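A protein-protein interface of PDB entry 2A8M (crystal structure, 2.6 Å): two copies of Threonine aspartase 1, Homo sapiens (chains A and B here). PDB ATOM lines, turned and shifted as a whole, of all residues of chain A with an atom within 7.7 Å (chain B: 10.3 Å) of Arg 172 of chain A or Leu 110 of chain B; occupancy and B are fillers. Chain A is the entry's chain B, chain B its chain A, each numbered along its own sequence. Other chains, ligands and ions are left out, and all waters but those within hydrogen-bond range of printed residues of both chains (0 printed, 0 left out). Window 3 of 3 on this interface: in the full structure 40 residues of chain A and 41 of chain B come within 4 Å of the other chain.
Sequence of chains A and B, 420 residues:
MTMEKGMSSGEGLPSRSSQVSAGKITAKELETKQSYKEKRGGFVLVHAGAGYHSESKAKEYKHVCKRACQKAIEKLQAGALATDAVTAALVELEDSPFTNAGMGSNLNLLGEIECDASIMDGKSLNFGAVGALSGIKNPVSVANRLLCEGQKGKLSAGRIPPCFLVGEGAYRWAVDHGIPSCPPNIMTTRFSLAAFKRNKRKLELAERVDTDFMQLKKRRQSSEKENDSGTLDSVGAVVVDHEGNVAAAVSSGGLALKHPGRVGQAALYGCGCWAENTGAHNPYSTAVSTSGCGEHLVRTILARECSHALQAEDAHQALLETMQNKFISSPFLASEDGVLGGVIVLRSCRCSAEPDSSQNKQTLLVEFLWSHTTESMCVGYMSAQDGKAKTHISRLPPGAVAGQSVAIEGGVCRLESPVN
O of Gly 261 of chain B lies within hydrogen-bond range of N of Val 166 of chain A (2.7 Å).
Printed residues of chain A that touch a printed residue of chain B: Leu 165, Val 166, Glu 168, Gly 169, Arg 172 and Trp 173.
Hydrophobic or aromatic side chains of chain A within 4 Å of the printed part of chain B: Leu 165, Val 166 and Trp 173.
Of the 17 printed residues of chain B, 6 touch a printed residue of chain A.
Hydrophobic or aromatic side chains of chain B within 4 Å of the printed part of chain A: Leu 109, Leu 110, His 259 and Pro 260.
Leu 133 of chain A touches none of the printed residues of chain B.
Of the printed residues of chain B, Leu 165 of chain A touches Gly 261 and Arg 262.
Of chain B, only His 259 and Pro 260 come within 4 Å of Gly 169 of chain A.
No residue of chain B comes within 4 Å of Ala 170 of chain A.
No residue of chain B comes within 4 Å of Ala 174 of chain A.
No residue of chain B comes within 4 Å of Val 175 of chain A.
Printed residues of chain A within 4 Å of Leu 109 of chain B: Arg 172.
Of chain A, only Arg 172 (2.9 Å) comes within 4 Å of Leu 110 of chain B.
Glu 114 of chain B touches none of the printed residues of chain A.
Printed residues of chain A within 4 Å of Pro 260 of chain B: Gly 169 (2.8 Å) and Arg 172 (3.6 Å).
Of the printed residues of chain A, Gly 261 of chain B touches Leu 165, Val 166 and Glu 168.
The nearest residue of chain B that does not touch Arg 172 of chain A is Lys 258 of chain B (6.9 Å).
The nearest residue of chain A that does not touch Leu 110 of chain B is Gly 169 of chain A (7.3 Å).
CA of Leu 165 of chain A touches O of Gly 261 of chain B, at 3.0 Å.
CD2 of Leu 165 of chain A touches CA of Arg 262 of chain B, 3.5 Å away.
Glu 168 of chain A touches Gly 261 of chain B (OE2 to CA, 3.8 Å).
Gly 169 of chain A touches His 259 of chain B (O to CE1, 3.1 Å).
Gly 169 of chain A touches Pro 260 of chain B (CA to O, 2.8 Å).
Leu 109 of chain B touches Arg 172 of chain A.
Arg 172 of chain A touches Leu 110 of chain B (NH1 to CD1, 2.9 Å).
His 259 of chain B touches Arg 172 of chain A (NE2 to NH2, 3.9 Å).
NH2 of Arg 172 of chain A touches CD of Pro 260 of chain B, at 3.6 Å.
His 259 of chain B touches Trp 173 of chain A (CD2 to CD1, 3.5 Å).
N of Leu 110 of chain B sits at hydrogen-bond distance from OD1 of Asn 108 of chain B.
The backbone NH (N) of Leu 109 of chain B lies within hydrogen-bond range of the backbone carbonyl oxygen (O) of Lys 258 of chain B (3.1 Å).
The side-chain carboxylate of Glu 114 of chain B sits at hydrogen-bond distance from the backbone NH of Gly 261 of chain B, at 2.9 Å.
A ring nitrogen (ND1) of His 177 of chain A lies within hydrogen-bond range of the backbone carbonyl oxygen of Trp 173 of chain A (2.9 Å).
No position is printed for both chains.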
ATOM      1  N   LEU A 133      -0.056  21.796 -33.735  1.00  0.00           N
ATOM      2  CA  LEU A 133       0.651  20.529 -33.843  1.00  0.00           C
ATOM      3  C   LEU A 133       0.303  19.757 -35.106  1.00  0.00           C
ATOM      4  O   LEU A 133      -0.850  19.396 -35.323  1.00  0.00           O
ATOM      5  CB  LEU A 133       0.333  19.652 -32.644  1.00  0.00           C
ATOM      6  CG  LEU A 133       0.890  18.234 -32.715  1.00  0.00           C
ATOM      7  CD1 LEU A 133       2.393  18.263 -32.555  1.00  0.00           C
ATOM      8  CD2 LEU A 133       0.264  17.395 -31.620  1.00  0.00           C
ATOM      9  N   SER A 134       1.316  19.501 -35.932  1.00  0.00           N
ATOM     10  CA  SER A 134       1.138  18.751 -37.172  1.00  0.00           C
ATOM     11  C   SER A 134       1.945  17.463 -37.043  1.00  0.00           C
ATOM     12  O   SER A 134       2.895  17.410 -36.263  1.00  0.00           O
ATOM     13  CB  SER A 134       1.657  19.556 -38.364  1.00  0.00           C
ATOM     14  OG  SER A 134       1.153  20.879 -38.342  1.00  0.00           O
ATOM     15  N   ILE A 136       0.761  14.428 -36.005  1.00  0.00           N
ATOM     16  CA  ILE A 136       0.277  13.503 -34.982  1.00  0.00           C
ATOM     17  C   ILE A 136      -1.195  13.213 -35.241  1.00  0.00           C
ATOM     18  O   ILE A 136      -2.002  14.133 -35.394  1.00  0.00           O
ATOM     19  CB  ILE A 136       0.422  14.084 -33.569  1.00  0.00           C
ATOM     20  CG1 ILE A 136       1.897  14.379 -33.273  1.00  0.00           C
ATOM     21  CG2 ILE A 136      -0.152  13.117 -32.552  1.00  0.00           C
ATOM     22  CD1 ILE A 136       2.789  13.150 -33.212  1.00  0.00           C
ATOM     23  N   LEU A 165       2.770  22.830 -24.971  1.00  0.00           N
ATOM     24  CA  LEU A 165       3.788  22.770 -26.011  1.00  0.00           C
ATOM     25  C   LEU A 165       3.184  23.075 -27.385  1.00  0.00           C
ATOM     26  O   LEU A 165       2.067  22.651 -27.682  1.00  0.00           O
ATOM     27  CB  LEU A 165       4.443  21.382 -26.049  1.00  0.00           C
ATOM     28  CG  LEU A 165       5.326  20.907 -24.886  1.00  0.00           C
ATOM     29  CD1 LEU A 165       6.030  19.634 -25.310  1.00  0.00           C
ATOM     30  CD2 LEU A 165       6.356  21.973 -24.489  1.00  0.00           C
ATOM     31  N   VAL A 166       3.915  23.813 -28.221  1.00  0.00           N
ATOM     32  CA  VAL A 166       3.419  24.134 -29.558  1.00  0.00           C
ATOM     33  C   VAL A 166       4.337  23.689 -30.700  1.00  0.00           C
ATOM     34  O   VAL A 166       5.531  23.443 -30.510  1.00  0.00           O
ATOM     35  CB  VAL A 166       3.121  25.655 -29.730  1.00  0.00           C
ATOM     36  CG1 VAL A 166       2.191  26.128 -28.611  1.00  0.00           C
ATOM     37  CG2 VAL A 166       4.413  26.464 -29.771  1.00  0.00           C
ATOM     38  N   GLY A 167       3.731  23.563 -31.879  1.00  0.00           N
ATOM     39  CA  GLY A 167       4.420  23.169 -33.097  1.00  0.00           C
ATOM     40  C   GLY A 167       5.541  22.147 -33.091  1.00  0.00           C
ATOM     41  O   GLY A 167       5.400  21.018 -32.632  1.00  0.00           O
ATOM     42  N   GLU A 168       6.662  22.569 -33.659  1.00  0.00           N
ATOM     43  CA  GLU A 168       7.862  21.761 -33.781  1.00  0.00           C
ATOM     44  C   GLU A 168       8.165  20.874 -32.566  1.00  0.00           C
ATOM     45  O   GLU A 168       8.107  19.653 -32.660  1.00  0.00           O
ATOM     46  CB  GLU A 168       9.029  22.694 -34.071  1.00  0.00           C
ATOM     47  CG  GLU A 168       8.601  24.169 -34.215  1.00  0.00           C
ATOM     48  CD  GLU A 168       8.306  24.865 -32.877  1.00  0.00           C
ATOM     49  OE1 GLU A 168       7.720  25.973 -32.914  1.00  0.00           O
ATOM     50  OE2 GLU A 168       8.669  24.323 -31.798  1.00  0.00           O
ATOM     51  N   GLY A 169       8.491  21.485 -31.434  1.00  0.00           N
ATOM     52  CA  GLY A 169       8.797  20.715 -30.245  1.00  0.00           C
ATOM     53  C   GLY A 169       7.646  19.845 -29.791  1.00  0.00           C
ATOM     54  O   GLY A 169       7.854  18.742 -29.275  1.00  0.00           O
ATOM     55  N   ALA A 170       6.424  20.339 -29.975  1.00  0.00           N
ATOM     56  CA  ALA A 170       5.237  19.585 -29.594  1.00  0.00           C
ATOM     57  C   ALA A 170       5.228  18.248 -30.332  1.00  0.00           C
ATOM     58  O   ALA A 170       4.795  17.233 -29.798  1.00  0.00           O
ATOM     59  CB  ALA A 170       3.985  20.379 -29.934  1.00  0.00           C
ATOM     60  N   TYR A 171       5.704  18.258 -31.571  1.00  0.00           N
ATOM     61  CA  TYR A 171       5.766  17.043 -32.365  1.00  0.00           C
ATOM     62  C   TYR A 171       6.883  16.148 -31.839  1.00  0.00           C
ATOM     63  O   TYR A 171       6.647  15.015 -31.421  1.00  0.00           O
ATOM     64  CB  TYR A 171       6.042  17.381 -33.826  1.00  0.00           C
ATOM     65  CG  TYR A 171       6.196  16.160 -34.695  1.00  0.00           C
ATOM     66  CD1 TYR A 171       5.118  15.307 -34.918  1.00  0.00           C
ATOM     67  CD2 TYR A 171       7.419  15.859 -35.298  1.00  0.00           C
ATOM     68  CE1 TYR A 171       5.245  14.181 -35.725  1.00  0.00           C
ATOM     69  CE2 TYR A 171       7.563  14.731 -36.108  1.00  0.00           C
ATOM     70  CZ  TYR A 171       6.467  13.895 -36.322  1.00  0.00           C
ATOM     71  OH  TYR A 171       6.580  12.796 -37.156  1.00  0.00           O
ATOM     72  N   ARG A 172       8.104  16.666 -31.873  1.00  0.00           N
ATOM     73  CA  ARG A 172       9.265  15.927 -31.393  1.00  0.00           C
ATOM     74  C   ARG A 172       8.947  15.228 -30.070  1.00  0.00           C
ATOM     75  O   ARG A 172       9.312  14.069 -29.856  1.00  0.00           O
ATOM     76  CB  ARG A 172      10.438  16.881 -31.190  1.00  0.00           C
ATOM     77  CG  ARG A 172      11.779  16.179 -31.143  1.00  0.00           C
ATOM     78  CD  ARG A 172      12.902  17.146 -30.810  1.00  0.00           C
ATOM     79  NE  ARG A 172      13.038  17.342 -29.372  1.00  0.00           N
ATOM     80  CZ  ARG A 172      14.004  18.059 -28.809  1.00  0.00           C
ATOM     81  NH1 ARG A 172      14.916  18.652 -29.569  1.00  0.00           N
ATOM     82  NH2 ARG A 172      14.074  18.165 -27.486  1.00  0.00           N
ATOM     83  N   TRP A 173       8.258  15.946 -29.189  1.00  0.00           N
ATOM     84  CA  TRP A 173       7.880  15.417 -27.887  1.00  0.00           C
ATOM     85  C   TRP A 173       6.913  14.249 -28.050  1.00  0.00           C
ATOM     86  O   TRP A 173       7.184  13.140 -27.594  1.00  0.00           O
ATOM     87  CB  TRP A 173       7.217  16.511 -27.056  1.00  0.00           C
ATOM     88  CG  TRP A 173       7.101  16.171 -25.604  1.00  0.00           C
ATOM     89  CD1 TRP A 173       8.010  16.443 -24.627  1.00  0.00           C
ATOM     90  CD2 TRP A 173       6.024  15.472 -24.965  1.00  0.00           C
ATOM     91  NE1 TRP A 173       7.571  15.958 -23.422  1.00  0.00           N
ATOM     92  CE2 TRP A 173       6.353  15.356 -23.601  1.00  0.00           C
ATOM     93  CE3 TRP A 173       4.814  14.932 -25.416  1.00  0.00           C
ATOM     94  CZ2 TRP A 173       5.515  14.723 -22.678  1.00  0.00           C
ATOM     95  CZ3 TRP A 173       3.979  14.302 -24.498  1.00  0.00           C
ATOM     96  CH2 TRP A 173       4.337  14.204 -23.146  1.00  0.00           C
ATOM     97  N   ALA A 174       5.781  14.507 -28.695  1.00  0.00           N
ATOM     98  CA  ALA A 174       4.778  13.470 -28.918  1.00  0.00           C
ATOM     99  C   ALA A 174       5.445  12.243 -29.513  1.00  0.00           C
ATOM    100  O   ALA A 174       5.028  11.113 -29.262  1.00  0.00           O
ATOM    101  CB  ALA A 174       3.692  13.979 -29.859  1.00  0.00           C
ATOM    102  N   VAL A 175       6.488  12.482 -30.302  1.00  0.00           N
ATOM    103  CA  VAL A 175       7.238  11.412 -30.950  1.00  0.00           C
ATOM    104  C   VAL A 175       8.115  10.632 -29.960  1.00  0.00           C
ATOM    105  O   VAL A 175       8.145   9.402 -29.991  1.00  0.00           O
ATOM    106  CB  VAL A 175       8.111  11.976 -32.088  1.00  0.00           C
ATOM    107  CG1 VAL A 175       9.106  10.931 -32.554  1.00  0.00           C
ATOM    108  CG2 VAL A 175       7.228  12.403 -33.242  1.00  0.00           C
ATOM    109  N   ASP A 176       8.830  11.344 -29.093  1.00  0.00           N
ATOM    110  CA  ASP A 176       9.675  10.686 -28.101  1.00  0.00           C
ATOM    111  C   ASP A 176       8.808  10.082 -26.997  1.00  0.00           C
ATOM    112  O   ASP A 176       9.293   9.777 -25.908  1.00  0.00           O
ATOM    113  CB  ASP A 176      10.677  11.669 -27.475  1.00  0.00           C
ATOM    114  CG  ASP A 176      11.716  12.174 -28.468  1.00  0.00           C
ATOM    115  OD1 ASP A 176      12.190  11.370 -29.301  1.00  0.00           O
ATOM    116  OD2 ASP A 176      12.074  13.374 -28.402  1.00  0.00           O
ATOM    117  N   HIS A 177       7.520   9.928 -27.276  1.00  0.00           N
ATOM    118  CA  HIS A 177       6.598   9.350 -26.307  1.00  0.00           C
ATOM    119  C   HIS A 177       5.666   8.381 -27.012  1.00  0.00           C
ATOM    120  O   HIS A 177       4.517   8.179 -26.609  1.00  0.00           O
ATOM    121  CB  HIS A 177       5.808  10.453 -25.590  1.00  0.00           C
ATOM    122  CG  HIS A 177       6.627  11.222 -24.600  1.00  0.00           C
ATOM    123  ND1 HIS A 177       7.689  12.018 -24.973  1.00  0.00           N
ATOM    124  CD2 HIS A 177       6.582  11.265 -23.248  1.00  0.00           C
ATOM    125  CE1 HIS A 177       8.264  12.515 -23.893  1.00  0.00           C
ATOM    126  NE2 HIS A 177       7.613  12.073 -22.833  1.00  0.00           N
ATOM    127  N   GLY A 178       6.193   7.784 -28.075  1.00  0.00           N
ATOM    128  CA  GLY A 178       5.449   6.815 -28.850  1.00  0.00           C
ATOM    129  C   GLY A 178       4.017   7.196 -29.135  1.00  0.00           C
ATOM    130  O   GLY A 178       3.104   6.418 -28.867  1.00  0.00           O
ATOM    131  N   ASN B 106      16.986  33.245 -22.225  1.00  0.00           N
ATOM    132  CA  ASN B 106      17.643  31.985 -21.916  1.00  0.00           C
ATOM    133  C   ASN B 106      17.547  31.105 -23.141  1.00  0.00           C
ATOM    134  O   ASN B 106      16.840  31.441 -24.073  1.00  0.00           O
ATOM    135  CB  ASN B 106      16.972  31.308 -20.716  1.00  0.00           C
ATOM    136  CG  ASN B 106      17.028  32.165 -19.469  1.00  0.00           C
ATOM    137  OD1 ASN B 106      17.929  32.997 -19.313  1.00  0.00           O
ATOM    138  ND2 ASN B 106      16.079  31.959 -18.567  1.00  0.00           N
ATOM    139  N   LEU B 107      18.248  29.979 -23.144  1.00  0.00           N
ATOM    140  CA  LEU B 107      18.232  29.080 -24.294  1.00  0.00           C
ATOM    141  C   LEU B 107      17.542  27.754 -23.993  1.00  0.00           C
ATOM    142  O   LEU B 107      17.719  27.170 -22.925  1.00  0.00           O
ATOM    143  CB  LEU B 107      19.669  28.829 -24.768  1.00  0.00           C
ATOM    144  CG  LEU B 107      20.435  29.950 -25.503  1.00  0.00           C
ATOM    145  CD1 LEU B 107      20.230  31.313 -24.845  1.00  0.00           C
ATOM    146  CD2 LEU B 107      21.904  29.588 -25.525  1.00  0.00           C
ATOM    147  N   ASN B 108      16.741  27.274 -24.936  1.00  0.00           N
ATOM    148  CA  ASN B 108      16.035  26.015 -24.740  1.00  0.00           C
ATOM    149  C   ASN B 108      17.015  24.850 -24.705  1.00  0.00           C
ATOM    150  O   ASN B 108      18.223  25.031 -24.853  1.00  0.00           O
ATOM    151  CB  ASN B 108      15.027  25.788 -25.868  1.00  0.00           C
ATOM    152  CG  ASN B 108      15.692  25.654 -27.229  1.00  0.00           C
ATOM    153  OD1 ASN B 108      16.913  25.505 -27.326  1.00  0.00           O
ATOM    154  ND2 ASN B 108      14.889  25.694 -28.288  1.00  0.00           N
ATOM    155  N   LEU B 109      16.475  23.649 -24.533  1.00  0.00           N
ATOM    156  CA  LEU B 109      17.274  22.435 -24.478  1.00  0.00           C
ATOM    157  C   LEU B 109      18.213  22.321 -25.678  1.00  0.00           C
ATOM    158  O   LEU B 109      19.301  21.766 -25.563  1.00  0.00           O
ATOM    159  CB  LEU B 109      16.356  21.219 -24.430  1.00  0.00           C
ATOM    160  CG  LEU B 109      17.051  19.895 -24.118  1.00  0.00           C
ATOM    161  CD1 LEU B 109      17.596  19.942 -22.699  1.00  0.00           C
ATOM    162  CD2 LEU B 109      16.067  18.738 -24.279  1.00  0.00           C
ATOM    163  N   LEU B 110      17.793  22.845 -26.830  1.00  0.00           N
ATOM    164  CA  LEU B 110      18.615  22.799 -28.042  1.00  0.00           C
ATOM    165  C   LEU B 110      19.364  24.116 -28.278  1.00  0.00           C
ATOM    166  O   LEU B 110      19.628  24.481 -29.418  1.00  0.00           O
ATOM    167  CB  LEU B 110      17.748  22.486 -29.271  1.00  0.00           C
ATOM    168  CG  LEU B 110      16.938  21.182 -29.282  1.00  0.00           C
ATOM    169  CD1 LEU B 110      16.035  21.141 -30.507  1.00  0.00           C
ATOM    170  CD2 LEU B 110      17.875  19.992 -29.271  1.00  0.00           C
ATOM    171  N   GLY B 111      19.690  24.833 -27.203  1.00  0.00           N
ATOM    172  CA  GLY B 111      20.414  26.087 -27.343  1.00  0.00           C
ATOM    173  C   GLY B 111      19.734  27.159 -28.184  1.00  0.00           C
ATOM    174  O   GLY B 111      20.234  28.281 -28.302  1.00  0.00           O
ATOM    175  N   GLU B 112      18.597  26.829 -28.779  1.00  0.00           N
ATOM    176  CA  GLU B 112      17.866  27.793 -29.586  1.00  0.00           C
ATOM    177  C   GLU B 112      17.081  28.751 -28.683  1.00  0.00           C
ATOM    178  O   GLU B 112      16.782  28.425 -27.528  1.00  0.00           O
ATOM    179  CB  GLU B 112      16.906  27.051 -30.516  1.00  0.00           C
ATOM    180  CG  GLU B 112      17.592  26.235 -31.595  1.00  0.00           C
ATOM    181  CD  GLU B 112      17.707  26.991 -32.906  1.00  0.00           C
ATOM    182  OE1 GLU B 112      16.663  27.188 -33.574  1.00  0.00           O
ATOM    183  OE2 GLU B 112      18.835  27.393 -33.271  1.00  0.00           O
ATOM    184  N   ILE B 113      16.752  29.931 -29.205  1.00  0.00           N
ATOM    185  CA  ILE B 113      15.987  30.919 -28.446  1.00  0.00           C
ATOM    186  C   ILE B 113      14.519  30.994 -28.891  1.00  0.00           C
ATOM    187  O   ILE B 113      14.222  30.943 -30.080  1.00  0.00           O
ATOM    188  CB  ILE B 113      16.626  32.320 -28.552  1.00  0.00           C
ATOM    189  CG1 ILE B 113      17.844  32.380 -27.636  1.00  0.00           C
ATOM    190  CG2 ILE B 113      15.623  33.404 -28.176  1.00  0.00           C
ATOM    191  CD1 ILE B 113      18.631  33.649 -27.769  1.00  0.00           C
ATOM    192  N   GLU B 114      13.611  31.093 -27.921  1.00  0.00           N
ATOM    193  CA  GLU B 114      12.182  31.183 -28.198  1.00  0.00           C
ATOM    194  C   GLU B 114      11.575  32.173 -27.222  1.00  0.00           C
ATOM    195  O   GLU B 114      11.672  31.992 -26.010  1.00  0.00           O
ATOM    196  CB  GLU B 114      11.500  29.831 -28.015  1.00  0.00           C
ATOM    197  CG  GLU B 114      12.329  28.674 -28.468  1.00  0.00           C
ATOM    198  CD  GLU B 114      11.495  27.463 -28.776  1.00  0.00           C
ATOM    199  OE1 GLU B 114      10.906  27.415 -29.880  1.00  0.00           O
ATOM    200  OE2 GLU B 114      11.421  26.562 -27.911  1.00  0.00           O
ATOM    201  N   LEU B 255      11.854  29.482 -19.473  1.00  0.00           N
ATOM    202  CA  LEU B 255      12.746  28.786 -18.552  1.00  0.00           C
ATOM    203  C   LEU B 255      13.980  28.331 -19.295  1.00  0.00           C
ATOM    204  O   LEU B 255      13.943  28.156 -20.510  1.00  0.00           O
ATOM    205  CB  LEU B 255      12.059  27.551 -17.965  1.00  0.00           C
ATOM    206  CG  LEU B 255      10.665  27.715 -17.355  1.00  0.00           C
ATOM    207  CD1 LEU B 255      10.133  26.347 -16.961  1.00  0.00           C
ATOM    208  CD2 LEU B 255      10.719  28.663 -16.160  1.00  0.00           C
ATOM    209  N   ALA B 256      15.071  28.128 -18.563  1.00  0.00           N
ATOM    210  CA  ALA B 256      16.303  27.667 -19.182  1.00  0.00           C
ATOM    211  C   ALA B 256      16.203  26.174 -19.486  1.00  0.00           C
ATOM    212  O   ALA B 256      15.655  25.402 -18.689  1.00  0.00           O
ATOM    213  CB  ALA B 256      17.468  27.933 -18.274  1.00  0.00           C
ATOM    214  N   LEU B 257      16.722  25.781 -20.646  1.00  0.00           N
ATOM    215  CA  LEU B 257      16.716  24.390 -21.074  1.00  0.00           C
ATOM    216  C   LEU B 257      15.312  23.856 -21.271  1.00  0.00           C
ATOM    217  O   LEU B 257      15.116  22.653 -21.411  1.00  0.00           O
ATOM    218  CB  LEU B 257      17.470  23.518 -20.064  1.00  0.00           C
ATOM    219  CG  LEU B 257      18.946  23.909 -19.855  1.00  0.00           C
ATOM    220  CD1 LEU B 257      19.599  22.998 -18.819  1.00  0.00           C
ATOM    221  CD2 LEU B 257      19.695  23.833 -21.191  1.00  0.00           C
ATOM    222  N   LYS B 258      14.334  24.756 -21.289  1.00  0.00           N
ATOM    223  CA  LYS B 258      12.945  24.368 -21.492  1.00  0.00           C
ATOM    224  C   LYS B 258      12.853  23.622 -22.813  1.00  0.00           C
ATOM    225  O   LYS B 258      13.516  23.988 -23.775  1.00  0.00           O
ATOM    226  CB  LYS B 258      12.054  25.606 -21.553  1.00  0.00           C
ATOM    227  CG  LYS B 258      12.378  26.521 -22.718  1.00  0.00           C
ATOM    228  CD  LYS B 258      11.517  27.770 -22.708  1.00  0.00           C
ATOM    229  CE  LYS B 258      11.761  28.578 -23.961  1.00  0.00           C
ATOM    230  NZ  LYS B 258      10.964  29.824 -23.990  1.00  0.00           N
ATOM    231  N   HIS B 259      12.033  22.578 -22.853  1.00  0.00           N
ATOM    232  CA  HIS B 259      11.861  21.802 -24.066  1.00  0.00           C
ATOM    233  C   HIS B 259      11.390  22.724 -25.189  1.00  0.00           C
ATOM    234  O   HIS B 259      10.600  23.634 -24.956  1.00  0.00           O
ATOM    235  CB  HIS B 259      10.841  20.703 -23.825  1.00  0.00           C
ATOM    236  CG  HIS B 259      10.550  19.877 -25.034  1.00  0.00           C
ATOM    237  ND1 HIS B 259      10.047  20.416 -26.199  1.00  0.00           N
ATOM    238  CD2 HIS B 259      10.679  18.550 -25.259  1.00  0.00           C
ATOM    239  CE1 HIS B 259       9.876  19.457 -27.090  1.00  0.00           C
ATOM    240  NE2 HIS B 259      10.251  18.314 -26.545  1.00  0.00           N
ATOM    241  N   PRO B 260      11.883  22.507 -26.427  1.00  0.00           N
ATOM    242  CA  PRO B 260      11.496  23.337 -27.575  1.00  0.00           C
ATOM    243  C   PRO B 260       9.992  23.329 -27.831  1.00  0.00           C
ATOM    244  O   PRO B 260       9.391  22.274 -28.039  1.00  0.00           O
ATOM    245  CB  PRO B 260      12.276  22.711 -28.735  1.00  0.00           C
ATOM    246  CG  PRO B 260      13.483  22.167 -28.081  1.00  0.00           C
ATOM    247  CD  PRO B 260      12.904  21.525 -26.834  1.00  0.00           C
ATOM    248  N   GLY B 261       9.386  24.508 -27.819  1.00  0.00           N
ATOM    249  CA  GLY B 261       7.962  24.584 -28.064  1.00  0.00           C
ATOM    250  C   GLY B 261       7.179  24.812 -26.793  1.00  0.00           C
ATOM    251  O   GLY B 261       5.948  24.730 -26.779  1.00  0.00           O
ATOM    252  N   ARG B 262       7.906  25.102 -25.719  1.00  0.00           N
ATOM    253  CA  ARG B 262       7.284  25.356 -24.440  1.00  0.00           C
ATOM    254  C   ARG B 262       6.960  26.827 -24.300  1.00  0.00           C
ATOM    255  O   ARG B 262       7.866  27.665 -24.242  1.00  0.00           O
ATOM    256  CB  ARG B 262       8.203  24.927 -23.299  1.00  0.00           C
ATOM    257  CG  ARG B 262       7.630  25.255 -21.936  1.00  0.00           C
ATOM    258  CD  ARG B 262       8.368  24.552 -20.833  1.00  0.00           C
ATOM    259  NE  ARG B 262       7.689  24.729 -19.554  1.00  0.00           N
ATOM    260  CZ  ARG B 262       7.884  23.959 -18.492  1.00  0.00           C
ATOM    261  NH1 ARG B 262       8.743  22.951 -18.545  1.00  0.00           N
ATOM    262  NH2 ARG B 262       7.210  24.192 -17.384  1.00  0.00           N
